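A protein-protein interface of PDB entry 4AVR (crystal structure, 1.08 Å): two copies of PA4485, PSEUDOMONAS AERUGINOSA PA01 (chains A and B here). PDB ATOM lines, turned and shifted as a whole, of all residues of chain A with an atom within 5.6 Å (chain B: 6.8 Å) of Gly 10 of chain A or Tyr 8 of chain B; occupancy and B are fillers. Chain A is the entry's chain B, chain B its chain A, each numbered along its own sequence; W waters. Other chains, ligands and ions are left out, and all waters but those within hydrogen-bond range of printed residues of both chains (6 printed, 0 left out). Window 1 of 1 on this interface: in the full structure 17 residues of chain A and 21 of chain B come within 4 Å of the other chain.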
ATOM      1  N   TYR A   8     -31.578  16.165  12.887  1.00  0.00           N
ATOM      2  CA  TYR A   8     -30.703  15.006  12.689  1.00  0.00           C
ATOM      3  C   TYR A   8     -30.346  14.310  13.997  1.00  0.00           C
ATOM      4  O   TYR A   8     -30.326  14.910  15.079  1.00  0.00           O
ATOM      5  CB  TYR A   8     -29.413  15.362  11.923  1.00  0.00           C
ATOM      6  CG  TYR A   8     -28.471  16.347  12.601  1.00  0.00           C
ATOM      7  CD1 TYR A   8     -27.488  15.904  13.475  1.00  0.00           C
ATOM      8  CD2 TYR A   8     -28.541  17.711  12.342  1.00  0.00           C
ATOM      9  CE1 TYR A   8     -26.605  16.791  14.084  1.00  0.00           C
ATOM     10  CE2 TYR A   8     -27.660  18.602  12.937  1.00  0.00           C
ATOM     11  CZ  TYR A   8     -26.698  18.133  13.810  1.00  0.00           C
ATOM     12  OH  TYR A   8     -25.813  19.008  14.406  1.00  0.00           O
ATOM     13  N   TYR A   9     -30.069  13.025  13.848  1.00  0.00           N
ATOM     14  CA  TYR A   9     -29.369  12.221  14.830  1.00  0.00           C
ATOM     15  C   TYR A   9     -27.873  12.482  14.712  1.00  0.00           C
ATOM     16  O   TYR A   9     -27.343  12.601  13.612  1.00  0.00           O
ATOM     17  CB  TYR A   9     -29.608  10.718  14.582  1.00  0.00           C
ATOM     18  CG  TYR A   9     -31.004  10.198  14.749  1.00  0.00           C
ATOM     19  CD1 TYR A   9     -31.943  10.311  13.728  1.00  0.00           C
ATOM     20  CD2 TYR A   9     -31.386   9.545  15.918  1.00  0.00           C
ATOM     21  CE1 TYR A   9     -33.237   9.824  13.877  1.00  0.00           C
ATOM     22  CE2 TYR A   9     -32.684   9.044  16.080  1.00  0.00           C
ATOM     23  CZ  TYR A   9     -33.605   9.196  15.060  1.00  0.00           C
ATOM     24  OH  TYR A   9     -34.890   8.702  15.197  1.00  0.00           O
ATOM     25  N   GLY A  10     -27.194  12.521  15.859  1.00  0.00           N
ATOM     26  CA  GLY A  10     -25.753  12.632  15.900  1.00  0.00           C
ATOM     27  C   GLY A  10     -25.153  11.253  16.052  1.00  0.00           C
ATOM     28  O   GLY A  10     -25.547  10.296  15.384  1.00  0.00           O
ATOM     29  N   SER A  11     -24.208  11.125  16.966  1.00  0.00           N
ATOM     30  CA  SER A  11     -23.624   9.830  17.299  1.00  0.00           C
ATOM     31  C   SER A  11     -24.001   9.337  18.696  1.00  0.00           C
ATOM     32  O   SER A  11     -23.704   8.192  19.019  1.00  0.00           O
ATOM     33  CB  SER A  11     -22.119   9.877  17.093  1.00  0.00           C
ATOM     34  OG  SER A  11     -21.571  10.984  17.756  1.00  0.00           O
ATOM     35  N   ARG A  12     -24.662  10.162  19.517  1.00  0.00           N
ATOM     36  CA  ARG A  12     -25.107   9.710  20.851  1.00  0.00           C
ATOM     37  C   ARG A  12     -25.973   8.448  20.742  1.00  0.00           C
ATOM     38  O   ARG A  12     -25.860   7.547  21.565  1.00  0.00           O
ATOM     39  CB  ARG A  12     -25.841  10.842  21.592  1.00  0.00           C
ATOM     40  CG  ARG A  12     -26.593  10.456  22.868  1.00  0.00           C
ATOM     41  CD  ARG A  12     -27.019  11.691  23.611  1.00  0.00           C
ATOM     42  NE  ARG A  12     -28.032  11.521  24.670  1.00  0.00           N
ATOM     43  CZ  ARG A  12     -27.780  11.374  25.978  1.00  0.00           C
ATOM     44  NH1 ARG A  12     -26.548  11.213  26.450  1.00  0.00           N
ATOM     45  NH2 ARG A  12     -28.794  11.346  26.821  1.00  0.00           N
ATOM     46  N   HIS A  13     -26.817   8.395  19.721  1.00  0.00           N
ATOM     47  CA  HIS A  13     -27.746   7.305  19.490  1.00  0.00           C
ATOM     48  C   HIS A  13     -27.104   6.099  18.826  1.00  0.00           C
ATOM     49  O   HIS A  13     -27.766   5.066  18.640  1.00  0.00           O
ATOM     50  CB  HIS A  13     -28.882   7.874  18.609  1.00  0.00           C
ATOM     51  CG  HIS A  13     -30.184   7.142  18.692  1.00  0.00           C
ATOM     52  ND1 HIS A  13     -30.948   7.165  19.804  1.00  0.00           N
ATOM     53  CD2 HIS A  13     -30.862   6.378  17.765  1.00  0.00           C
ATOM     54  CE1 HIS A  13     -32.054   6.433  19.603  1.00  0.00           C
ATOM     55  NE2 HIS A  13     -32.023   5.967  18.347  1.00  0.00           N
ATOM     56  N   ALA A  14     -25.831   6.194  18.437  1.00  0.00           N
ATOM     57  CA  ALA A  14     -25.191   5.120  17.690  1.00  0.00           C
ATOM     58  C   ALA A  14     -25.262   3.817  18.444  1.00  0.00           C
ATOM     59  O   ALA A  14     -24.942   3.746  19.641  1.00  0.00           O
ATOM     60  CB  ALA A  14     -23.739   5.451  17.387  1.00  0.00           C
ATOM     61  N   TYR A  24     -28.905   1.920  14.850  1.00  0.00           N
ATOM     62  CA  TYR A  24     -28.599   3.174  14.196  1.00  0.00           C
ATOM     63  C   TYR A  24     -27.092   3.292  13.971  1.00  0.00           C
ATOM     64  O   TYR A  24     -26.293   3.064  14.877  1.00  0.00           O
ATOM     65  CB  TYR A  24     -29.131   4.354  15.023  1.00  0.00           C
ATOM     66  CG  TYR A  24     -28.590   5.683  14.572  1.00  0.00           C
ATOM     67  CD1 TYR A  24     -28.863   6.185  13.305  1.00  0.00           C
ATOM     68  CD2 TYR A  24     -27.778   6.436  15.398  1.00  0.00           C
ATOM     69  CE1 TYR A  24     -28.326   7.393  12.891  1.00  0.00           C
ATOM     70  CE2 TYR A  24     -27.247   7.637  14.988  1.00  0.00           C
ATOM     71  CZ  TYR A  24     -27.513   8.116  13.726  1.00  0.00           C
ATOM     72  OH  TYR A  24     -26.985   9.307  13.293  1.00  0.00           O
ATOM     73  N   PRO A  26     -24.453   6.110  12.548  1.00  0.00           N
ATOM     74  CA  PRO A  26     -24.354   7.496  12.109  1.00  0.00           C
ATOM     75  C   PRO A  26     -23.671   7.665  10.759  1.00  0.00           C
ATOM     76  O   PRO A  26     -23.820   8.723  10.156  1.00  0.00           O
ATOM     77  CB  PRO A  26     -23.542   8.184  13.220  1.00  0.00           C
ATOM     78  CG  PRO A  26     -22.987   7.115  14.062  1.00  0.00           C
ATOM     79  CD  PRO A  26     -23.756   5.864  13.827  1.00  0.00           C
ATOM     80  N   ARG A  73     -26.496  11.274  10.966  1.00  0.00           N
ATOM     81  CA  ARG A  73     -25.419  12.247  11.052  1.00  0.00           C
ATOM     82  C   ARG A  73     -24.766  12.453   9.686  1.00  0.00           C
ATOM     83  O   ARG A  73     -24.534  13.588   9.268  1.00  0.00           O
ATOM     84  CB  ARG A  73     -24.368  11.774  12.069  1.00  0.00           C
ATOM     85  CG  ARG A  73     -23.288  12.810  12.364  1.00  0.00           C
ATOM     86  CD  ARG A  73     -21.947  12.198  12.777  1.00  0.00           C
ATOM     87  NE  ARG A  73     -21.393  11.311  11.755  1.00  0.00           N
ATOM     88  CZ  ARG A  73     -20.849  11.714  10.597  1.00  0.00           C
ATOM     89  NH1 ARG A  73     -20.739  13.013  10.322  1.00  0.00           N
ATOM     90  NH2 ARG A  73     -20.425  10.832   9.702  1.00  0.00           N
ATOM     91  N   ILE A  82     -25.386  20.538   9.841  1.00  0.00           N
ATOM     92  CA  ILE A  82     -24.879  20.216  11.179  1.00  0.00           C
ATOM     93  C   ILE A  82     -24.913  21.438  12.096  1.00  0.00           C
ATOM     94  O   ILE A  82     -25.396  21.366  13.225  1.00  0.00           O
ATOM     95  CB  ILE A  82     -23.459  19.602  11.118  1.00  0.00           C
ATOM     96  CG1 ILE A  82     -23.462  18.259  10.399  1.00  0.00           C
ATOM     97  CG2 ILE A  82     -22.876  19.474  12.525  1.00  0.00           C
ATOM     98  CD1 ILE A  82     -24.046  17.144  11.196  1.00  0.00           C
ATOM     99  N   ALA B   6     -16.140   9.061  22.851  1.00  0.00           N
ATOM    100  CA  ALA B   6     -17.041  10.224  22.905  1.00  0.00           C
ATOM    101  C   ALA B   6     -17.918  10.224  21.667  1.00  0.00           C
ATOM    102  O   ALA B   6     -17.486   9.861  20.575  1.00  0.00           O
ATOM    103  CB  ALA B   6     -16.273  11.538  22.957  1.00  0.00           C
ATOM    104  N   SER B   7     -19.147  10.696  21.855  1.00  0.00           N
ATOM    105  CA  SER B   7     -20.087  10.968  20.773  1.00  0.00           C
ATOM    106  C   SER B   7     -20.582  12.398  20.911  1.00  0.00           C
ATOM    107  O   SER B   7     -20.246  13.073  21.876  1.00  0.00           O
ATOM    108  CB  SER B   7     -21.289  10.028  20.872  1.00  0.00           C
ATOM    109  OG  SER B   7     -22.166  10.472  21.893  1.00  0.00           O
ATOM    110  N   TYR B   8     -21.427  12.833  19.970  1.00  0.00           N
ATOM    111  CA  TYR B   8     -22.116  14.107  20.133  1.00  0.00           C
ATOM    112  C   TYR B   8     -23.597  13.981  19.838  1.00  0.00           C
ATOM    113  O   TYR B   8     -24.047  13.124  19.070  1.00  0.00           O
ATOM    114  CB  TYR B   8     -21.463  15.247  19.355  1.00  0.00           C
ATOM    115  CG  TYR B   8     -21.524  15.228  17.845  1.00  0.00           C
ATOM    116  CD1 TYR B   8     -22.565  15.833  17.159  1.00  0.00           C
ATOM    117  CD2 TYR B   8     -20.478  14.689  17.104  1.00  0.00           C
ATOM    118  CE1 TYR B   8     -22.567  15.895  15.763  1.00  0.00           C
ATOM    119  CE2 TYR B   8     -20.443  14.748  15.729  1.00  0.00           C
ATOM    120  CZ  TYR B   8     -21.495  15.341  15.067  1.00  0.00           C
ATOM    121  OH  TYR B   8     -21.475  15.424  13.687  1.00  0.00           O
ATOM    122  N   TYR B   9     -24.364  14.831  20.504  1.00  0.00           N
ATOM    123  CA  TYR B   9     -25.815  14.853  20.356  1.00  0.00           C
ATOM    124  C   TYR B   9     -26.241  15.309  18.960  1.00  0.00           C
ATOM    125  O   TYR B   9     -25.693  16.246  18.398  1.00  0.00           O
ATOM    126  CB  TYR B   9     -26.428  15.861  21.310  1.00  0.00           C
ATOM    127  CG  TYR B   9     -26.482  15.538  22.789  1.00  0.00           C
ATOM    128  CD1 TYR B   9     -25.339  15.550  23.568  1.00  0.00           C
ATOM    129  CD2 TYR B   9     -27.695  15.304  23.429  1.00  0.00           C
ATOM    130  CE1 TYR B   9     -25.398  15.333  24.931  1.00  0.00           C
ATOM    131  CE2 TYR B   9     -27.760  15.100  24.794  1.00  0.00           C
ATOM    132  CZ  TYR B   9     -26.606  15.113  25.542  1.00  0.00           C
ATOM    133  OH  TYR B   9     -26.647  14.928  26.905  1.00  0.00           O
ATOM    134  N   GLY B  10     -27.289  14.687  18.453  1.00  0.00           N
ATOM    135  CA  GLY B  10     -27.990  15.237  17.303  1.00  0.00           C
ATOM    136  C   GLY B  10     -28.841  16.435  17.672  1.00  0.00           C
ATOM    137  O   GLY B  10     -29.328  16.572  18.805  1.00  0.00           O
ATOM    138  N   SER B  11     -29.124  17.263  16.680  1.00  0.00           N
ATOM    139  CA  SER B  11     -29.971  18.437  16.863  1.00  0.00           C
ATOM    140  C   SER B  11     -31.395  18.056  17.134  1.00  0.00           C
ATOM    141  O   SER B  11     -32.148  18.916  17.612  1.00  0.00           O
ATOM    142  CB  SER B  11     -30.024  19.288  15.581  1.00  0.00           C
ATOM    143  OG  SER B  11     -30.593  18.547  14.521  1.00  0.00           O
ATOM    144  N   ARG B  12     -31.793  16.822  16.856  1.00  0.00           N
ATOM    145  CA  ARG B  12     -33.146  16.384  17.157  1.00  0.00           C
ATOM    146  C   ARG B  12     -33.446  16.522  18.651  1.00  0.00           C
ATOM    147  O   ARG B  12     -34.606  16.636  19.026  1.00  0.00           O
ATOM    148  CB  ARG B  12     -33.363  14.959  16.698  1.00  0.00           C
ATOM    149  CG  ARG B  12     -32.534  13.950  17.453  1.00  0.00           C
ATOM    150  CD  ARG B  12     -32.715  12.571  16.849  1.00  0.00           C
ATOM    151  NE  ARG B  12     -34.066  12.038  16.985  1.00  0.00           N
ATOM    152  CZ  ARG B  12     -34.489  11.232  17.956  1.00  0.00           C
ATOM    153  NH1 ARG B  12     -33.677  10.842  18.944  1.00  0.00           N
ATOM    154  NH2 ARG B  12     -35.750  10.806  17.926  1.00  0.00           N
ATOM    155  N   HIS B  13     -32.395  16.525  19.482  1.00  0.00           N
ATOM    156  CA  HIS B  13     -32.528  16.653  20.936  1.00  0.00           C
ATOM    157  C   HIS B  13     -32.656  18.080  21.397  1.00  0.00           C
ATOM    158  O   HIS B  13     -32.971  18.314  22.567  1.00  0.00           O
ATOM    159  CB  HIS B  13     -31.334  16.025  21.646  1.00  0.00           C
ATOM    160  CG  HIS B  13     -31.142  14.571  21.331  1.00  0.00           C
ATOM    161  ND1 HIS B  13     -31.996  13.618  21.734  1.00  0.00           N
ATOM    162  CD2 HIS B  13     -30.160  13.927  20.573  1.00  0.00           C
ATOM    163  CE1 HIS B  13     -31.570  12.425  21.277  1.00  0.00           C
ATOM    164  NE2 HIS B  13     -30.443  12.615  20.582  1.00  0.00           N
ATOM    165  N   TYR B  24     -31.572  20.704  26.279  1.00  0.00           N
ATOM    166  CA  TYR B  24     -30.322  20.528  25.559  1.00  0.00           C
ATOM    167  C   TYR B  24     -30.129  21.677  24.554  1.00  0.00           C
ATOM    168  O   TYR B  24     -31.042  21.994  23.783  1.00  0.00           O
ATOM    169  CB  TYR B  24     -30.265  19.157  24.853  1.00  0.00           C
ATOM    170  CG  TYR B  24     -29.084  19.092  23.889  1.00  0.00           C
ATOM    171  CD1 TYR B  24     -27.771  19.241  24.342  1.00  0.00           C
ATOM    172  CD2 TYR B  24     -29.281  18.957  22.533  1.00  0.00           C
ATOM    173  CE1 TYR B  24     -26.716  19.271  23.451  1.00  0.00           C
ATOM    174  CE2 TYR B  24     -28.225  18.982  21.636  1.00  0.00           C
ATOM    175  CZ  TYR B  24     -26.933  19.155  22.098  1.00  0.00           C
ATOM    176  OH  TYR B  24     -25.862  19.225  21.248  1.00  0.00           O
ATOM    177  N   ARG B  67     -18.720   3.684  25.602  1.00  0.00           N
ATOM    178  CA  ARG B  67     -18.934   5.118  25.390  1.00  0.00           C
ATOM    179  C   ARG B  67     -18.923   5.788  26.761  1.00  0.00           C
ATOM    180  O   ARG B  67     -19.694   5.416  27.638  1.00  0.00           O
ATOM    181  CB  ARG B  67     -20.250   5.362  24.617  1.00  0.00           C
ATOM    182  CG  ARG B  67     -20.436   6.799  24.093  1.00  0.00           C
ATOM    183  CD  ARG B  67     -21.534   6.905  23.040  1.00  0.00           C
ATOM    184  NE  ARG B  67     -21.309   5.995  21.922  1.00  0.00           N
ATOM    185  CZ  ARG B  67     -22.271   5.391  21.222  1.00  0.00           C
ATOM    186  NH1 ARG B  67     -23.558   5.570  21.524  1.00  0.00           N
ATOM    187  NH2 ARG B  67     -21.925   4.547  20.249  1.00  0.00           N
ATOM    188  N   ILE B  69     -18.692   9.504  27.262  1.00  0.00           N
ATOM    189  CA  ILE B  69     -19.234  10.859  27.338  1.00  0.00           C
ATOM    190  C   ILE B  69     -19.905  11.204  26.024  1.00  0.00           C
ATOM    191  O   ILE B  69     -19.455  10.777  24.972  1.00  0.00           O
ATOM    192  CB  ILE B  69     -18.111  11.861  27.710  1.00  0.00           C
ATOM    193  CG1 ILE B  69     -18.652  13.209  28.190  1.00  0.00           C
ATOM    194  CG2 ILE B  69     -17.080  12.011  26.594  1.00  0.00           C
ATOM    195  CD1 ILE B  69     -17.621  14.041  28.927  1.00  0.00           C
ATOM    196  N   ASP B  70     -21.004  11.955  26.098  1.00  0.00           N
ATOM    197  CA  ASP B  70     -21.669  12.509  24.924  1.00  0.00           C
ATOM    198  C   ASP B  70     -21.635  14.021  25.049  1.00  0.00           C
ATOM    199  O   ASP B  70     -22.069  14.542  26.067  1.00  0.00           O
ATOM    200  CB  ASP B  70     -23.135  12.056  24.849  1.00  0.00           C
ATOM    201  CG  ASP B  70     -23.307  10.533  24.855  1.00  0.00           C
ATOM    202  OD1 ASP B  70     -22.415   9.791  24.383  1.00  0.00           O
ATOM    203  OD2 ASP B  70     -24.354  10.073  25.346  1.00  0.00           O
ATOM    204  N   VAL B  71     -21.128  14.723  24.034  1.00  0.00           N
ATOM    205  CA  VAL B  71     -20.913  16.166  24.139  1.00  0.00           C
ATOM    206  C   VAL B  71     -21.842  16.942  23.201  1.00  0.00           C
ATOM    207  O   VAL B  71     -22.387  16.404  22.241  1.00  0.00           O
ATOM    208  CB  VAL B  71     -19.426  16.537  23.870  1.00  0.00           C
ATOM    209  CG1 VAL B  71     -18.505  15.751  24.797  1.00  0.00           C
ATOM    210  CG2 VAL B  71     -19.055  16.325  22.410  1.00  0.00           C
ATOM    211  N   SER B  72     -21.999  18.227  23.492  1.00  0.00           N
ATOM    212  CA  SER B  72     -22.779  19.105  22.633  1.00  0.00           C
ATOM    213  C   SER B  72     -22.120  19.293  21.268  1.00  0.00           C
ATOM    214  O   SER B  72     -20.929  19.044  21.086  1.00  0.00           O
ATOM    215  CB  SER B  72     -22.929  20.463  23.279  1.00  0.00           C
ATOM    216  OG  SER B  72     -21.655  21.100  23.327  1.00  0.00           O
ATOM    217  N   ARG B  73     -22.898  19.802  20.315  1.00  0.00           N
ATOM    218  CA  ARG B  73     -22.349  20.110  18.997  1.00  0.00           C
ATOM    219  C   ARG B  73     -21.172  21.073  19.078  1.00  0.00           C
ATOM    220  O   ARG B  73     -20.146  20.872  18.421  1.00  0.00           O
ATOM    221  CB  ARG B  73     -23.439  20.686  18.089  1.00  0.00           C
ATOM    222  CG  ARG B  73     -23.007  20.745  16.620  1.00  0.00           C
ATOM    223  CD  ARG B  73     -22.952  22.092  15.999  1.00  0.00           C
ATOM    224  NE  ARG B  73     -23.870  23.035  16.502  1.00  0.00           N
ATOM    225  CZ  ARG B  73     -23.669  24.221  17.066  1.00  0.00           C
ATOM    226  NH1 ARG B  73     -22.496  24.846  17.265  1.00  0.00           N
ATOM    227  NH2 ARG B  73     -24.776  24.789  17.436  1.00  0.00           N
ATOM    228  N   ALA B  75     -19.132  21.601  21.550  1.00  0.00           N
ATOM    229  CA  ALA B  75     -17.972  20.902  22.104  1.00  0.00           C
ATOM    230  C   ALA B  75     -17.332  19.996  21.051  1.00  0.00           C
ATOM    231  O   ALA B  75     -16.102  19.894  20.974  1.00  0.00           O
ATOM    232  CB  ALA B  75     -18.367  20.108  23.339  1.00  0.00           C
ATOM    233  N   ALA B  76     -18.154  19.324  20.255  1.00  0.00           N
ATOM    234  CA  ALA B  76     -17.646  18.466  19.188  1.00  0.00           C
ATOM    235  C   ALA B  76     -16.839  19.255  18.167  1.00  0.00           C
ATOM    236  O   ALA B  76     -15.817  18.782  17.664  1.00  0.00           O
ATOM    237  CB  ALA B  76     -18.769  17.731  18.515  1.00  0.00           C
ATOM    238  N   GLU B  77     -17.280  20.473  17.865  1.00  0.00           N
ATOM    239  CA  GLU B  77     -16.494  21.368  17.000  1.00  0.00           C
ATOM    240  C   GLU B  77     -15.127  21.663  17.608  1.00  0.00           C
ATOM    241  O   GLU B  77     -14.107  21.588  16.922  1.00  0.00           O
ATOM    242  CB  GLU B  77     -17.253  22.676  16.737  1.00  0.00           C
ATOM    243  CG  GLU B  77     -18.490  22.466  15.882  1.00  0.00           C
ATOM    244  CD  GLU B  77     -19.410  23.653  15.778  1.00  0.00           C
ATOM    245  OE1 GLU B  77     -19.488  24.497  16.684  1.00  0.00           O
ATOM    246  OE2 GLU B  77     -20.218  23.667  14.825  1.00  0.00           O
ATOM    247  N   MET B  81     -14.331  16.723  16.028  1.00  0.00           N
ATOM    248  CA  MET B  81     -14.957  15.405  15.853  1.00  0.00           C
ATOM    249  C   MET B  81     -16.279  15.431  15.073  1.00  0.00           C
ATOM    250  O   MET B  81     -16.991  14.429  15.039  1.00  0.00           O
ATOM    251  CB  MET B  81     -15.124  14.688  17.195  1.00  0.00           C
ATOM    252  CG  MET B  81     -16.140  15.294  18.110  1.00  0.00           C
ATOM    253  SD  MET B  81     -16.212  14.531  19.747  1.00  0.00           S
ATOM    254  CE  MET B  81     -17.227  13.126  19.406  1.00  0.00           C
ATOM    255  N   ILE B  82     -16.604  16.547  14.434  1.00  0.00           N
ATOM    256  CA  ILE B  82     -17.886  16.639  13.724  1.00  0.00           C
ATOM    257  C   ILE B  82     -17.972  15.603  12.605  1.00  0.00           C
ATOM    258  O   ILE B  82     -18.992  14.916  12.473  1.00  0.00           O
ATOM    259  CB  ILE B  82     -18.135  18.066  13.201  1.00  0.00           C
ATOM    260  CG1 ILE B  82     -18.379  19.019  14.378  1.00  0.00           C
ATOM    261  CG2 ILE B  82     -19.286  18.107  12.206  1.00  0.00           C
ATOM    262  CD1 ILE B  82     -19.714  18.809  15.083  1.00  0.00           C
ATOM    263  N   ARG B  83     -16.926  15.503  11.791  1.00  0.00           N
ATOM    264  CA  ARG B  83     -16.938  14.561  10.670  1.00  0.00           C
ATOM    265  C   ARG B  83     -16.687  13.133  11.105  1.00  0.00           C
ATOM    266  O   ARG B  83     -17.296  12.213  10.559  1.00  0.00           O
ATOM    267  CB  ARG B  83     -15.947  14.970   9.588  1.00  0.00           C
ATOM    268  CG  ARG B  83     -16.391  16.206   8.846  1.00  0.00           C
ATOM    269  CD  ARG B  83     -15.269  16.771   7.984  1.00  0.00           C
ATOM    270  NE  ARG B  83     -14.712  15.837   7.003  1.00  0.00           N
ATOM    271  CZ  ARG B  83     -13.762  16.160   6.122  1.00  0.00           C
ATOM    272  NH1 ARG B  83     -13.257  17.389   6.100  1.00  0.00           N
ATOM    273  NH2 ARG B  83     -13.313  15.262   5.253  1.00  0.00           N
ATOM    274  N   SER B  84     -15.808  12.915  12.085  1.00  0.00           N
ATOM    275  CA  SER B  84     -15.557  11.553  12.552  1.00  0.00           C
ATOM    276  C   SER B  84     -16.745  10.984  13.310  1.00  0.00           C
ATOM    277  O   SER B  84     -16.925   9.762  13.336  1.00  0.00           O
ATOM    278  CB  SER B  84     -14.313  11.477  13.425  1.00  0.00           C
ATOM    279  OG  SER B  84     -14.430  12.226  14.607  1.00  0.00           O
ATOM    280  N   GLY B  85     -17.542  11.843  13.934  1.00  0.00           N
ATOM    281  CA  GLY B  85     -18.745  11.423  14.655  1.00  0.00           C
ATOM    282  C   GLY B  85     -18.451  10.961  16.069  1.00  0.00           C
ATOM    283  O   GLY B  85     -19.084  11.393  17.029  1.00  0.00           O
ATOM    284  N   VAL B  86     -17.501  10.048  16.178  1.00  0.00           N
ATOM    285  CA  VAL B  86     -17.011   9.586  17.447  1.00  0.00           C
ATOM    286  C   VAL B  86     -15.500   9.717  17.479  1.00  0.00           C
ATOM    287  O   VAL B  86     -14.844   9.891  16.450  1.00  0.00           O
ATOM    288  CB  VAL B  86     -17.417   8.130  17.664  1.00  0.00           C
ATOM    289  CG1 VAL B  86     -18.930   8.011  17.780  1.00  0.00           C
ATOM    290  CG2 VAL B  86     -16.861   7.223  16.565  1.00  0.00           C
HETATM  291  O   HOH W   1     -24.861   7.451  24.253  1.00  0.00           O
HETATM  292  O   HOH W   2     -18.115  11.866   7.792  1.00  0.00           O
HETATM  293  O   HOH W   3     -35.670   7.568  17.515  1.00  0.00           O
HETATM  294  O   HOH W   4     -17.300   9.410   9.878  1.00  0.00           O
HETATM  295  O   HOH W   5     -36.916  10.789  15.298  1.00  0.00           O
HETATM  296  O   HOH W   6     -20.198   8.669  13.041  1.00  0.00           O
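The side-chain hydroxyl (OG) of Ser 7 of chain B sits close to the backbone NH (N) of Arg 12 of chain A.
N of Tyr 8 of chain B lies within hydrogen-bond range of OG of Ser 11 of chain A (2.9 Å).
The backbone carbonyl oxygen (O) of Tyr 8 of chain B is in hydrogen-bond range of the backbone NH (N) of Arg 12 of chain A (3.1 Å).
OG of Ser 11 of chain B lies within hydrogen-bond range of N of Tyr 8 of chain A (3.1 Å).
The backbone carbonyl oxygen of Tyr 8 of chain A is in hydrogen-bond range of the backbone NH of Arg 12 of chain B (3.0 Å).
The guanidinium group of Arg 67 of chain B is in hydrogen-bond range of the backbone carbonyl oxygen of Arg 12 of chain A (3.0 Å).
The backbone carbonyl oxygen (O) of Ala 14 of chain A lies within hydrogen-bond range of the guanidinium group (NH1) of Arg 67 of chain B (3.0 Å).
OD2 of Asp 70 of chain B is in salt-bridge range of NH1 of Arg 12 of chain A (2.7 Å).
The backbone carbonyl oxygen (O) of Ile 82 of chain B lies within hydrogen-bond range of the guanidinium group (NH1) of Arg 73 of chain A, at 3.4 Å.
The backbone carbonyl oxygen of Gly 85 of chain B sits at hydrogen-bond distance from the side-chain hydroxyl of Ser 11 of chain A (2.6 Å).
N of Gly 10 of chain B lies close to N of Gly 10 of chain A.
The backbone NH (N) of Arg 73 of chain B lies within hydrogen-bond range of the side-chain hydroxyl (OH) of Tyr 24 of chain B (3.2 Å).
O of Tyr 9 of chain A lies close to OH of Tyr 24 of chain A.
The side-chain hydroxyl of Tyr 24 of chain A sits at hydrogen-bond distance from the backbone NH of Arg 73 of chain A, at 3.1 Å.
Tyr 9 of chain A touches Gly 10 of chain B (C to CA, 3.8 Å).
NH1 of Arg 67 of chain B touches O of Ser 11 of chain A, 3.6 Å away.
Tyr 9 of chain B touches Arg 12 of chain A (CE2 to NE, 3.6 Å).
CA of Gly 85 of chain B touches CD of Arg 73 of chain A, 3.8 Å away.
CD1 of Ile 82 of chain A touches OH of Tyr 8 of chain B, at 3.97 Å.
Arg 73 of chain B touches Ile 82 of chain A (CD to O, 3.8 Å).
Gly 10 of chain A touches just these residues of chain B: Tyr 8 and Gly 10.
Of chain A, only Gly 10, Ser 11, Arg 12, Arg 73 and Ile 82 come within 4 Å of Tyr 8 of chain B.
Printed residues of chain B within 4 Å of Tyr 8 of chain A: Gly 10, Ser 11, Arg 12 and Arg 73.
Of the printed residues of chain A, Gly 85 of chain B touches Ser 11 (2.6 Å) and Arg 73 (3.8 Å).
Printed residues of chain B within 4 Å of Arg 73 of chain A: Tyr 8, Ile 82, Arg 83 and Gly 85.
The nearest residue of chain A that does not touch Tyr 8 of chain B is Tyr 8 of chain A (4.5 Å).
The nearest printed residue of chain B that does not touch Tyr 8 of chain A is Tyr 9 of chain B (4.4 Å).
Of the 11 printed residues of chain A, 8 touch a printed residue of chain B.
Of the 24 printed residues of chain B, 13 touch a printed residue of chain A.
Printed residues of chain B that touch a printed residue of chain A: Ser 7, Tyr 8, Tyr 9, Gly 10, Ser 11, Arg 12, Arg 67, Asp 70, Arg 73, Ile 82, Arg 83, Gly 85 and Val 86.
Hydrophobic or aromatic side chains of chain B within 4 Å of the printed part of chain A: Tyr 8, Tyr 9, Ile 82 and Val 86.
Among the printed residues, Asp or Glu carboxylates within 4 Å of a Lys or Arg side-chain nitrogen of the other chain: Arg 12 of chain A with Asp 70 of chain B (2.7 Å).
Tyr 8 of chain A touches Gly 10 of chain B, and with the chains exchanged Gly 10 of chain A touches Tyr 8 of chain B.
Positions printed for both chains: 8, 9, 10, 11, 12, 13, 24, 73 and 82.
Of the 26 pairs that touch across the chains among the printed residues, 14 have their exchanged pair printed and touching as well.
Water W3 lies within hydrogen-bond range of the side-chain hydroxyl of Tyr 9 of chain A (2.7 Å) and the guanidinium group of Arg 12 of chain B (3.3 Å).
Water W5 lies within hydrogen-bond range of NH2 of Arg 12 of chain B (2.9 Å) and OH of Tyr 9 of chain A (2.9 Å).
Water W2 bridges the backbone carbonyl oxygen of Arg 83 of chain B (2.9 Å) and the guanidinium group of Arg 73 of chain A (3.2 Å).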
